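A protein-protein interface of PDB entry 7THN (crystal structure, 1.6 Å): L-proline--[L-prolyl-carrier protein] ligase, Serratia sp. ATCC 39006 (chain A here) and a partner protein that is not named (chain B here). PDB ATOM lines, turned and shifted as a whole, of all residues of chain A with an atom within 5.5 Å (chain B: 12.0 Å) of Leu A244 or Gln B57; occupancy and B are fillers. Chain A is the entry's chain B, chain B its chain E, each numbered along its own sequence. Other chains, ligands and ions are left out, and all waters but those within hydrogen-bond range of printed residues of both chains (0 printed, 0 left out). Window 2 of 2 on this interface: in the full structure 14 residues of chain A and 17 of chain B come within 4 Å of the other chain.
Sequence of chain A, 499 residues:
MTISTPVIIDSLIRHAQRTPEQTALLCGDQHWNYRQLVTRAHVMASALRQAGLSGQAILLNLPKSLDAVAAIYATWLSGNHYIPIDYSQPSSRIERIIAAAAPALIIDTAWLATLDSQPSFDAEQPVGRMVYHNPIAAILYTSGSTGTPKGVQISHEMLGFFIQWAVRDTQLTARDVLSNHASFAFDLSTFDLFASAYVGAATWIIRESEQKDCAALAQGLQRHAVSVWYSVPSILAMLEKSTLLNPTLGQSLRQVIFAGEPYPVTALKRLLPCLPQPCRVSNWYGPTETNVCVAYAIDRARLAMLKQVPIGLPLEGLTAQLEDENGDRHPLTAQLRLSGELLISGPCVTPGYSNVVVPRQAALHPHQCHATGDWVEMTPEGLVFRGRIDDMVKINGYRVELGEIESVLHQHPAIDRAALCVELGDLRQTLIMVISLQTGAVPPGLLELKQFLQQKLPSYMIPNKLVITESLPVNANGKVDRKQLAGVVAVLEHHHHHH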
ATOM      1  N   CYS A 214      -8.343  25.090  12.326  1.00  0.00           N
ATOM      2  CA  CYS A 214      -9.362  24.293  11.603  1.00  0.00           C
ATOM      3  C   CYS A 214     -10.619  25.109  11.285  1.00  0.00           C
ATOM      4  O   CYS A 214     -11.080  25.059  10.152  1.00  0.00           O
ATOM      5  CB  CYS A 214      -9.696  23.009  12.316  1.00  0.00           C
ATOM      6  SG  CYS A 214      -8.337  21.819  12.158  1.00  0.00           S
ATOM      7  N   ALA A 215     -11.080  25.972  12.184  1.00  0.00           N
ATOM      8  CA  ALA A 215     -12.216  26.862  11.854  1.00  0.00           C
ATOM      9  C   ALA A 215     -11.862  27.843  10.732  1.00  0.00           C
ATOM     10  O   ALA A 215     -12.699  28.020   9.852  1.00  0.00           O
ATOM     11  CB  ALA A 215     -12.674  27.604  13.093  1.00  0.00           C
ATOM     12  N   ALA A 218     -11.678  25.786   7.427  1.00  0.00           N
ATOM     13  CA  ALA A 218     -13.022  25.379   6.963  1.00  0.00           C
ATOM     14  C   ALA A 218     -13.757  26.588   6.405  1.00  0.00           C
ATOM     15  O   ALA A 218     -14.374  26.488   5.302  1.00  0.00           O
ATOM     16  CB  ALA A 218     -13.801  24.736   8.070  1.00  0.00           C
ATOM     17  N   LEU A 239      -8.623  18.419  10.414  1.00  0.00           N
ATOM     18  CA  LEU A 239      -9.895  18.954   9.882  1.00  0.00           C
ATOM     19  C   LEU A 239     -10.990  17.901  10.096  1.00  0.00           C
ATOM     20  O   LEU A 239     -12.105  18.292  10.533  1.00  0.00           O
ATOM     21  CB  LEU A 239      -9.709  19.323   8.409  1.00  0.00           C
ATOM     22  CG  LEU A 239      -9.013  20.653   8.161  1.00  0.00           C
ATOM     23  CD1 LEU A 239      -8.502  20.749   6.732  1.00  0.00           C
ATOM     24  CD2 LEU A 239      -9.968  21.774   8.476  1.00  0.00           C
ATOM     25  N   GLU A 240     -10.720  16.626   9.838  1.00  0.00           N
ATOM     26  CA  GLU A 240     -11.701  15.542  10.114  1.00  0.00           C
ATOM     27  C   GLU A 240     -12.091  15.580  11.606  1.00  0.00           C
ATOM     28  O   GLU A 240     -13.325  15.605  11.917  1.00  0.00           O
ATOM     29  CB  GLU A 240     -11.156  14.178   9.712  1.00  0.00           C
ATOM     30  CG  GLU A 240     -12.112  12.977   9.953  1.00  0.00           C
ATOM     31  CD  GLU A 240     -12.390  12.416  11.368  1.00  0.00           C
ATOM     32  OE1 GLU A 240     -13.567  12.078  11.685  1.00  0.00           O
ATOM     33  OE2 GLU A 240     -11.468  12.230  12.123  1.00  0.00           O
ATOM     34  N   SER A 242     -11.931  17.880  13.778  1.00  0.00           N
ATOM     35  CA  SER A 242     -12.531  19.153  14.233  1.00  0.00           C
ATOM     36  C   SER A 242     -14.055  19.059  14.233  1.00  0.00           C
ATOM     37  O   SER A 242     -14.628  19.922  14.882  1.00  0.00           O
ATOM     38  CB  SER A 242     -12.133  20.338  13.432  1.00  0.00           C
ATOM     39  OG  SER A 242     -12.607  20.272  12.097  1.00  0.00           O
ATOM     40  N   THR A 243     -14.627  18.191  13.389  1.00  0.00           N
ATOM     41  CA  THR A 243     -16.081  18.073  13.051  1.00  0.00           C
ATOM     42  C   THR A 243     -16.525  19.210  12.109  1.00  0.00           C
ATOM     43  O   THR A 243     -17.736  19.260  11.792  1.00  0.00           O
ATOM     44  CB  THR A 243     -16.988  17.938  14.290  1.00  0.00           C
ATOM     45  OG1 THR A 243     -17.211  19.256  14.806  1.00  0.00           O
ATOM     46  CG2 THR A 243     -16.414  16.979  15.313  1.00  0.00           C
ATOM     47  N   LEU A 244     -15.635  20.082  11.643  1.00  0.00           N
ATOM     48  CA  LEU A 244     -16.025  21.277  10.881  1.00  0.00           C
ATOM     49  C   LEU A 244     -16.009  20.991   9.378  1.00  0.00           C
ATOM     50  O   LEU A 244     -16.607  21.746   8.663  1.00  0.00           O
ATOM     51  CB  LEU A 244     -15.142  22.451  11.221  1.00  0.00           C
ATOM     52  CG  LEU A 244     -15.094  22.837  12.700  1.00  0.00           C
ATOM     53  CD1 LEU A 244     -14.254  24.074  12.853  1.00  0.00           C
ATOM     54  CD2 LEU A 244     -16.495  23.087  13.236  1.00  0.00           C
ATOM     55  N   LEU A 245     -15.374  19.922   8.932  1.00  0.00           N
ATOM     56  CA  LEU A 245     -15.283  19.633   7.481  1.00  0.00           C
ATOM     57  C   LEU A 245     -16.389  18.654   7.105  1.00  0.00           C
ATOM     58  O   LEU A 245     -16.489  17.571   7.710  1.00  0.00           O
ATOM     59  CB  LEU A 245     -13.917  19.020   7.165  1.00  0.00           C
ATOM     60  CG  LEU A 245     -13.669  18.658   5.705  1.00  0.00           C
ATOM     61  CD1 LEU A 245     -13.683  19.893   4.843  1.00  0.00           C
ATOM     62  CD2 LEU A 245     -12.359  17.914   5.548  1.00  0.00           C
ATOM     63  N   ASN A 246     -17.200  19.026   6.113  1.00  0.00           N
ATOM     64  CA  ASN A 246     -18.292  18.146   5.641  1.00  0.00           C
ATOM     65  C   ASN A 246     -18.453  18.382   4.146  1.00  0.00           C
ATOM     66  O   ASN A 246     -17.939  19.369   3.599  1.00  0.00           O
ATOM     67  CB  ASN A 246     -19.566  18.372   6.484  1.00  0.00           C
ATOM     68  CG  ASN A 246     -20.103  19.772   6.247  1.00  0.00           C
ATOM     69  OD1 ASN A 246     -20.566  20.048   5.137  1.00  0.00           O
ATOM     70  ND2 ASN A 246     -20.036  20.639   7.253  1.00  0.00           N
ATOM     71  N   LEU A 249     -20.133  22.112   3.204  1.00  0.00           N
ATOM     72  CA  LEU A 249     -19.132  23.191   3.358  1.00  0.00           C
ATOM     73  C   LEU A 249     -18.031  23.018   2.288  1.00  0.00           C
ATOM     74  O   LEU A 249     -17.575  24.037   1.734  1.00  0.00           O
ATOM     75  CB  LEU A 249     -18.526  23.088   4.762  1.00  0.00           C
ATOM     76  CG  LEU A 249     -17.405  24.089   5.045  1.00  0.00           C
ATOM     77  CD1 LEU A 249     -17.582  24.757   6.385  1.00  0.00           C
ATOM     78  CD2 LEU A 249     -16.060  23.404   4.995  1.00  0.00           C
ATOM     79  N   ILE B  39      -4.819  18.922  19.604  1.00  0.00           N
ATOM     80  CA  ILE B  39      -5.654  19.984  20.208  1.00  0.00           C
ATOM     81  C   ILE B  39      -7.077  19.467  20.520  1.00  0.00           C
ATOM     82  O   ILE B  39      -7.625  19.849  21.565  1.00  0.00           O
ATOM     83  CB  ILE B  39      -5.673  21.226  19.310  1.00  0.00           C
ATOM     84  CG1 ILE B  39      -6.479  22.339  19.977  1.00  0.00           C
ATOM     85  CG2 ILE B  39      -6.170  20.931  17.893  1.00  0.00           C
ATOM     86  CD1 ILE B  39      -6.161  23.717  19.463  1.00  0.00           C
ATOM     87  N   PHE B  40      -7.717  18.705  19.630  1.00  0.00           N
ATOM     88  CA  PHE B  40      -9.138  18.290  19.830  1.00  0.00           C
ATOM     89  C   PHE B  40      -9.269  17.322  21.011  1.00  0.00           C
ATOM     90  O   PHE B  40     -10.378  17.305  21.649  1.00  0.00           O
ATOM     91  CB  PHE B  40      -9.729  17.770  18.517  1.00  0.00           C
ATOM     92  CG  PHE B  40      -9.741  18.863  17.499  1.00  0.00           C
ATOM     93  CD1 PHE B  40     -10.489  20.002  17.721  1.00  0.00           C
ATOM     94  CD2 PHE B  40      -8.891  18.823  16.406  1.00  0.00           C
ATOM     95  CE1 PHE B  40     -10.430  21.073  16.845  1.00  0.00           C
ATOM     96  CE2 PHE B  40      -8.850  19.882  15.521  1.00  0.00           C
ATOM     97  CZ  PHE B  40      -9.604  21.011  15.754  1.00  0.00           C
ATOM     98  N   VAL B  43      -9.642  19.776  23.798  1.00  0.00           N
ATOM     99  CA  VAL B  43     -10.988  20.426  23.719  1.00  0.00           C
ATOM    100  C   VAL B  43     -12.009  19.474  24.347  1.00  0.00           C
ATOM    101  O   VAL B  43     -12.841  19.936  25.140  1.00  0.00           O
ATOM    102  CB  VAL B  43     -11.360  20.806  22.270  1.00  0.00           C
ATOM    103  CG1 VAL B  43     -12.758  21.420  22.176  1.00  0.00           C
ATOM    104  CG2 VAL B  43     -10.324  21.766  21.674  1.00  0.00           C
ATOM    105  N   ARG B  47     -14.360  20.208  27.498  1.00  0.00           N
ATOM    106  CA  ARG B  47     -15.841  20.292  27.381  1.00  0.00           C
ATOM    107  C   ARG B  47     -16.463  19.369  28.440  1.00  0.00           C
ATOM    108  O   ARG B  47     -17.379  19.796  29.170  1.00  0.00           O
ATOM    109  CB  ARG B  47     -16.224  19.863  25.965  1.00  0.00           C
ATOM    110  CG  ARG B  47     -17.718  19.868  25.699  1.00  0.00           C
ATOM    111  CD  ARG B  47     -18.000  19.216  24.359  1.00  0.00           C
ATOM    112  NE  ARG B  47     -17.475  19.998  23.248  1.00  0.00           N
ATOM    113  CZ  ARG B  47     -16.470  19.635  22.477  1.00  0.00           C
ATOM    114  NH1 ARG B  47     -15.873  18.472  22.673  1.00  0.00           N
ATOM    115  NH2 ARG B  47     -16.086  20.418  21.481  1.00  0.00           N
ATOM    116  N   SER B  53     -20.815  24.125  26.830  1.00  0.00           N
ATOM    117  CA  SER B  53     -20.650  23.811  25.393  1.00  0.00           C
ATOM    118  C   SER B  53     -19.464  24.594  24.833  1.00  0.00           C
ATOM    119  O   SER B  53     -19.319  25.803  25.163  1.00  0.00           O
ATOM    120  CB  SER B  53     -21.938  24.064  24.641  1.00  0.00           C
ATOM    121  OG  SER B  53     -22.948  23.222  25.177  1.00  0.00           O
ATOM    122  N   ILE B  54     -18.637  23.920  24.042  1.00  0.00           N
ATOM    123  CA  ILE B  54     -17.433  24.512  23.398  1.00  0.00           C
ATOM    124  C   ILE B  54     -17.528  24.203  21.904  1.00  0.00           C
ATOM    125  O   ILE B  54     -17.206  23.080  21.511  1.00  0.00           O
ATOM    126  CB  ILE B  54     -16.142  23.987  24.045  1.00  0.00           C
ATOM    127  CG1 ILE B  54     -16.135  24.266  25.553  1.00  0.00           C
ATOM    128  CG2 ILE B  54     -14.924  24.591  23.359  1.00  0.00           C
ATOM    129  CD1 ILE B  54     -14.825  23.916  26.239  1.00  0.00           C
ATOM    130  N   GLY B  55     -18.068  25.143  21.137  1.00  0.00           N
ATOM    131  CA  GLY B  55     -18.184  25.003  19.675  1.00  0.00           C
ATOM    132  C   GLY B  55     -16.966  25.585  18.982  1.00  0.00           C
ATOM    133  O   GLY B  55     -16.785  26.807  19.011  1.00  0.00           O
ATOM    134  N   MET B  56     -16.192  24.755  18.312  1.00  0.00           N
ATOM    135  CA  MET B  56     -14.934  25.198  17.671  1.00  0.00           C
ATOM    136  C   MET B  56     -15.241  26.051  16.426  1.00  0.00           C
ATOM    137  O   MET B  56     -14.298  26.683  15.923  1.00  0.00           O
ATOM    138  CB  MET B  56     -14.029  24.005  17.354  1.00  0.00           C
ATOM    139  CG  MET B  56     -13.248  23.492  18.602  1.00  0.00           C
ATOM    140  SD  MET B  56     -12.527  24.796  19.671  1.00  0.00           S
ATOM    141  CE  MET B  56     -11.019  25.083  18.737  1.00  0.00           C
ATOM    142  N   GLN B  57     -16.498  26.162  15.983  1.00  0.00           N
ATOM    143  CA  GLN B  57     -16.870  27.123  14.903  1.00  0.00           C
ATOM    144  C   GLN B  57     -16.542  28.551  15.366  1.00  0.00           C
ATOM    145  O   GLN B  57     -16.116  29.360  14.516  1.00  0.00           O
ATOM    146  CB  GLN B  57     -18.359  27.061  14.547  1.00  0.00           C
ATOM    147  CG  GLN B  57     -18.763  25.758  13.881  1.00  0.00           C
ATOM    148  N   GLU B  58     -16.757  28.844  16.650  1.00  0.00           N
ATOM    149  CA  GLU B  58     -16.853  30.228  17.212  1.00  0.00           C
ATOM    150  C   GLU B  58     -15.774  30.488  18.285  1.00  0.00           C
ATOM    151  O   GLU B  58     -15.692  31.642  18.758  1.00  0.00           O
ATOM    152  CB  GLU B  58     -18.255  30.464  17.797  1.00  0.00           C
ATOM    153  CG  GLU B  58     -18.646  29.501  18.924  1.00  0.00           C
ATOM    154  N   ILE B  59     -14.968  29.487  18.672  1.00  0.00           N
ATOM    155  CA  ILE B  59     -13.987  29.623  19.791  1.00  0.00           C
ATOM    156  C   ILE B  59     -12.561  29.531  19.252  1.00  0.00           C
ATOM    157  O   ILE B  59     -12.175  28.431  18.756  1.00  0.00           O
ATOM    158  CB  ILE B  59     -14.243  28.564  20.870  1.00  0.00           C
ATOM    159  CG1 ILE B  59     -15.625  28.803  21.483  1.00  0.00           C
ATOM    160  CG2 ILE B  59     -13.120  28.556  21.904  1.00  0.00           C
ATOM    161  CD1 ILE B  59     -16.088  27.722  22.358  1.00  0.00           C
ATOM    162  N   HIS B  60     -11.780  30.606  19.452  1.00  0.00           N
ATOM    163  CA  HIS B  60     -10.405  30.743  18.893  1.00  0.00           C
ATOM    164  C   HIS B  60      -9.528  29.648  19.481  1.00  0.00           C
ATOM    165  O   HIS B  60      -9.562  29.429  20.701  1.00  0.00           O
ATOM    166  CB  HIS B  60      -9.789  32.111  19.222  1.00  0.00           C
ATOM    167  CG  HIS B  60      -8.700  32.482  18.271  1.00  0.00           C
ATOM    168  ND1 HIS B  60      -7.438  31.896  18.329  1.00  0.00           N
ATOM    169  CD2 HIS B  60      -8.683  33.320  17.208  1.00  0.00           C
ATOM    170  CE1 HIS B  60      -6.681  32.390  17.360  1.00  0.00           C
ATOM    171  NE2 HIS B  60      -7.417  33.267  16.653  1.00  0.00           N
ATOM    172  N   PRO B  61      -8.700  28.949  18.666  1.00  0.00           N
ATOM    173  CA  PRO B  61      -7.822  27.910  19.232  1.00  0.00           C
ATOM    174  C   PRO B  61      -6.748  28.400  20.221  1.00  0.00           C
ATOM    175  O   PRO B  61      -6.229  27.601  21.005  1.00  0.00           O
ATOM    176  CB  PRO B  61      -7.135  27.286  18.004  1.00  0.00           C
ATOM    177  CG  PRO B  61      -7.347  28.311  16.873  1.00  0.00           C
ATOM    178  CD  PRO B  61      -8.632  29.057  17.204  1.00  0.00           C
ATOM    179  N   ALA B  62      -6.375  29.690  20.174  1.00  0.00           N
ATOM    180  CA  ALA B  62      -5.432  30.289  21.140  1.00  0.00           C
ATOM    181  C   ALA B  62      -5.949  30.048  22.556  1.00  0.00           C
ATOM    182  O   ALA B  62      -5.184  30.074  23.505  1.00  0.00           O
ATOM    183  CB  ALA B  62      -5.295  31.770  20.890  1.00  0.00           C
ATOM    184  N   ASN B  63      -7.253  29.843  22.731  1.00  0.00           N
ATOM    185  CA  ASN B  63      -7.810  29.586  24.074  1.00  0.00           C
ATOM    186  C   ASN B  63      -7.217  28.303  24.677  1.00  0.00           C
ATOM    187  O   ASN B  63      -7.340  28.208  25.872  1.00  0.00           O
ATOM    188  CB  ASN B  63      -9.338  29.478  24.103  1.00  0.00           C
ATOM    189  CG  ASN B  63      -9.989  30.823  23.886  1.00  0.00           C
ATOM    190  OD1 ASN B  63     -10.049  31.649  24.816  1.00  0.00           O
ATOM    191  ND2 ASN B  63     -10.463  31.045  22.679  1.00  0.00           N
ATOM    192  N   PHE B  64      -6.644  27.390  23.912  1.00  0.00           N
ATOM    193  CA  PHE B  64      -6.050  26.117  24.419  1.00  0.00           C
ATOM    194  C   PHE B  64      -4.528  26.153  24.624  1.00  0.00           C
ATOM    195  O   PHE B  64      -3.922  25.092  24.882  1.00  0.00           O
ATOM    196  CB  PHE B  64      -6.484  24.955  23.520  1.00  0.00           C
ATOM    197  CG  PHE B  64      -7.981  24.926  23.438  1.00  0.00           C
ATOM    198  CD1 PHE B  64      -8.722  24.236  24.382  1.00  0.00           C
ATOM    199  CD2 PHE B  64      -8.652  25.698  22.508  1.00  0.00           C
ATOM    200  CE1 PHE B  64     -10.103  24.242  24.324  1.00  0.00           C
ATOM    201  CE2 PHE B  64     -10.036  25.713  22.461  1.00  0.00           C
ATOM    202  CZ  PHE B  64     -10.756  25.024  23.399  1.00  0.00           C
ATOM    203  N   LEU B  73     -11.314  30.950  29.367  1.00  0.00           N
ATOM    204  CA  LEU B  73     -12.365  30.692  28.375  1.00  0.00           C
ATOM    205  C   LEU B  73     -13.628  30.139  29.053  1.00  0.00           C
ATOM    206  O   LEU B  73     -14.759  30.548  28.673  1.00  0.00           O
ATOM    207  CB  LEU B  73     -11.858  29.685  27.349  1.00  0.00           C
ATOM    208  CG  LEU B  73     -12.956  29.127  26.455  1.00  0.00           C
ATOM    209  CD1 LEU B  73     -13.549  30.196  25.542  1.00  0.00           C
ATOM    210  CD2 LEU B  73     -12.528  27.916  25.693  1.00  0.00           C
ATOM    211  N   LEU B  77     -17.509  31.591  29.154  1.00  0.00           N
ATOM    212  CA  LEU B  77     -18.665  30.797  28.637  1.00  0.00           C
ATOM    213  C   LEU B  77     -19.713  30.647  29.750  1.00  0.00           C
ATOM    214  O   LEU B  77     -20.884  30.594  29.420  1.00  0.00           O
ATOM    215  CB  LEU B  77     -18.202  29.430  28.116  1.00  0.00           C
ATOM    216  CG  LEU B  77     -17.400  29.449  26.818  1.00  0.00           C
ATOM    217  CD1 LEU B  77     -16.838  28.069  26.497  1.00  0.00           C
ATOM    218  CD2 LEU B  77     -18.217  29.977  25.655  1.00  0.00           C
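Hydrophobic or aromatic side chains of chain B within 4 Å of the printed part of chain A: Phe B40. Along chain B the printed residues that touch a printed residue of chain A span positions 40 to 57. Of the 11 printed residues of chain A, 4 touch a printed residue of chain B. Printed residues of chain A that touch a printed residue of chain B: Cys A214, Ala A215, Ser A242 and Leu A244. Hydrophobic or aromatic side chains of chain A within 4 Å of the printed part of chain B: Ala A215 and Leu A244. Among the printed residues, no Asp or Glu carboxylate lies within 4 Å of a Lys or Arg side-chain nitrogen of the other chain.
Of the printed residues of chain B, Cys A214 touches Phe B40 (3.9 Å). Ser A242 touches just one residue of chain B: Phe B40 (3.5 Å). Leu A244 touches just one residue of chain B: Gln B57 (3.6 Å). Leu A249 touches none of the printed residues of chain B. Of the printed residues of chain A, Phe B40 touches Cys A214 and Ser A242. Of the printed residues of chain A, Met B56 touches Ala A215 (3.4 Å). Of chain A, only Leu A244 (3.6 Å) comes within 4 Å of Gln B57. His B60 touches none of the printed residues of chain A. The nearest residue of chain B that does not touch Leu A244 is Met B56 (4.03 Å).
The backbone carbonyl oxygen (O) of Leu A239 lies within hydrogen-bond range of the side-chain hydroxyl (OG) of Ser A242 (2.6 Å). The side-chain hydroxyl (OG) of Ser A242 lies within hydrogen-bond range of the backbone NH (N) of Leu A244, at 3.1 Å.
SG of Cys A214 touches CZ of Phe B40, at 3.9 Å. Ala A215 touches Met B56. Phe B40 touches Ser A242. CD2 of Leu A244 touches CG of Gln B57, 3.6 Å away.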
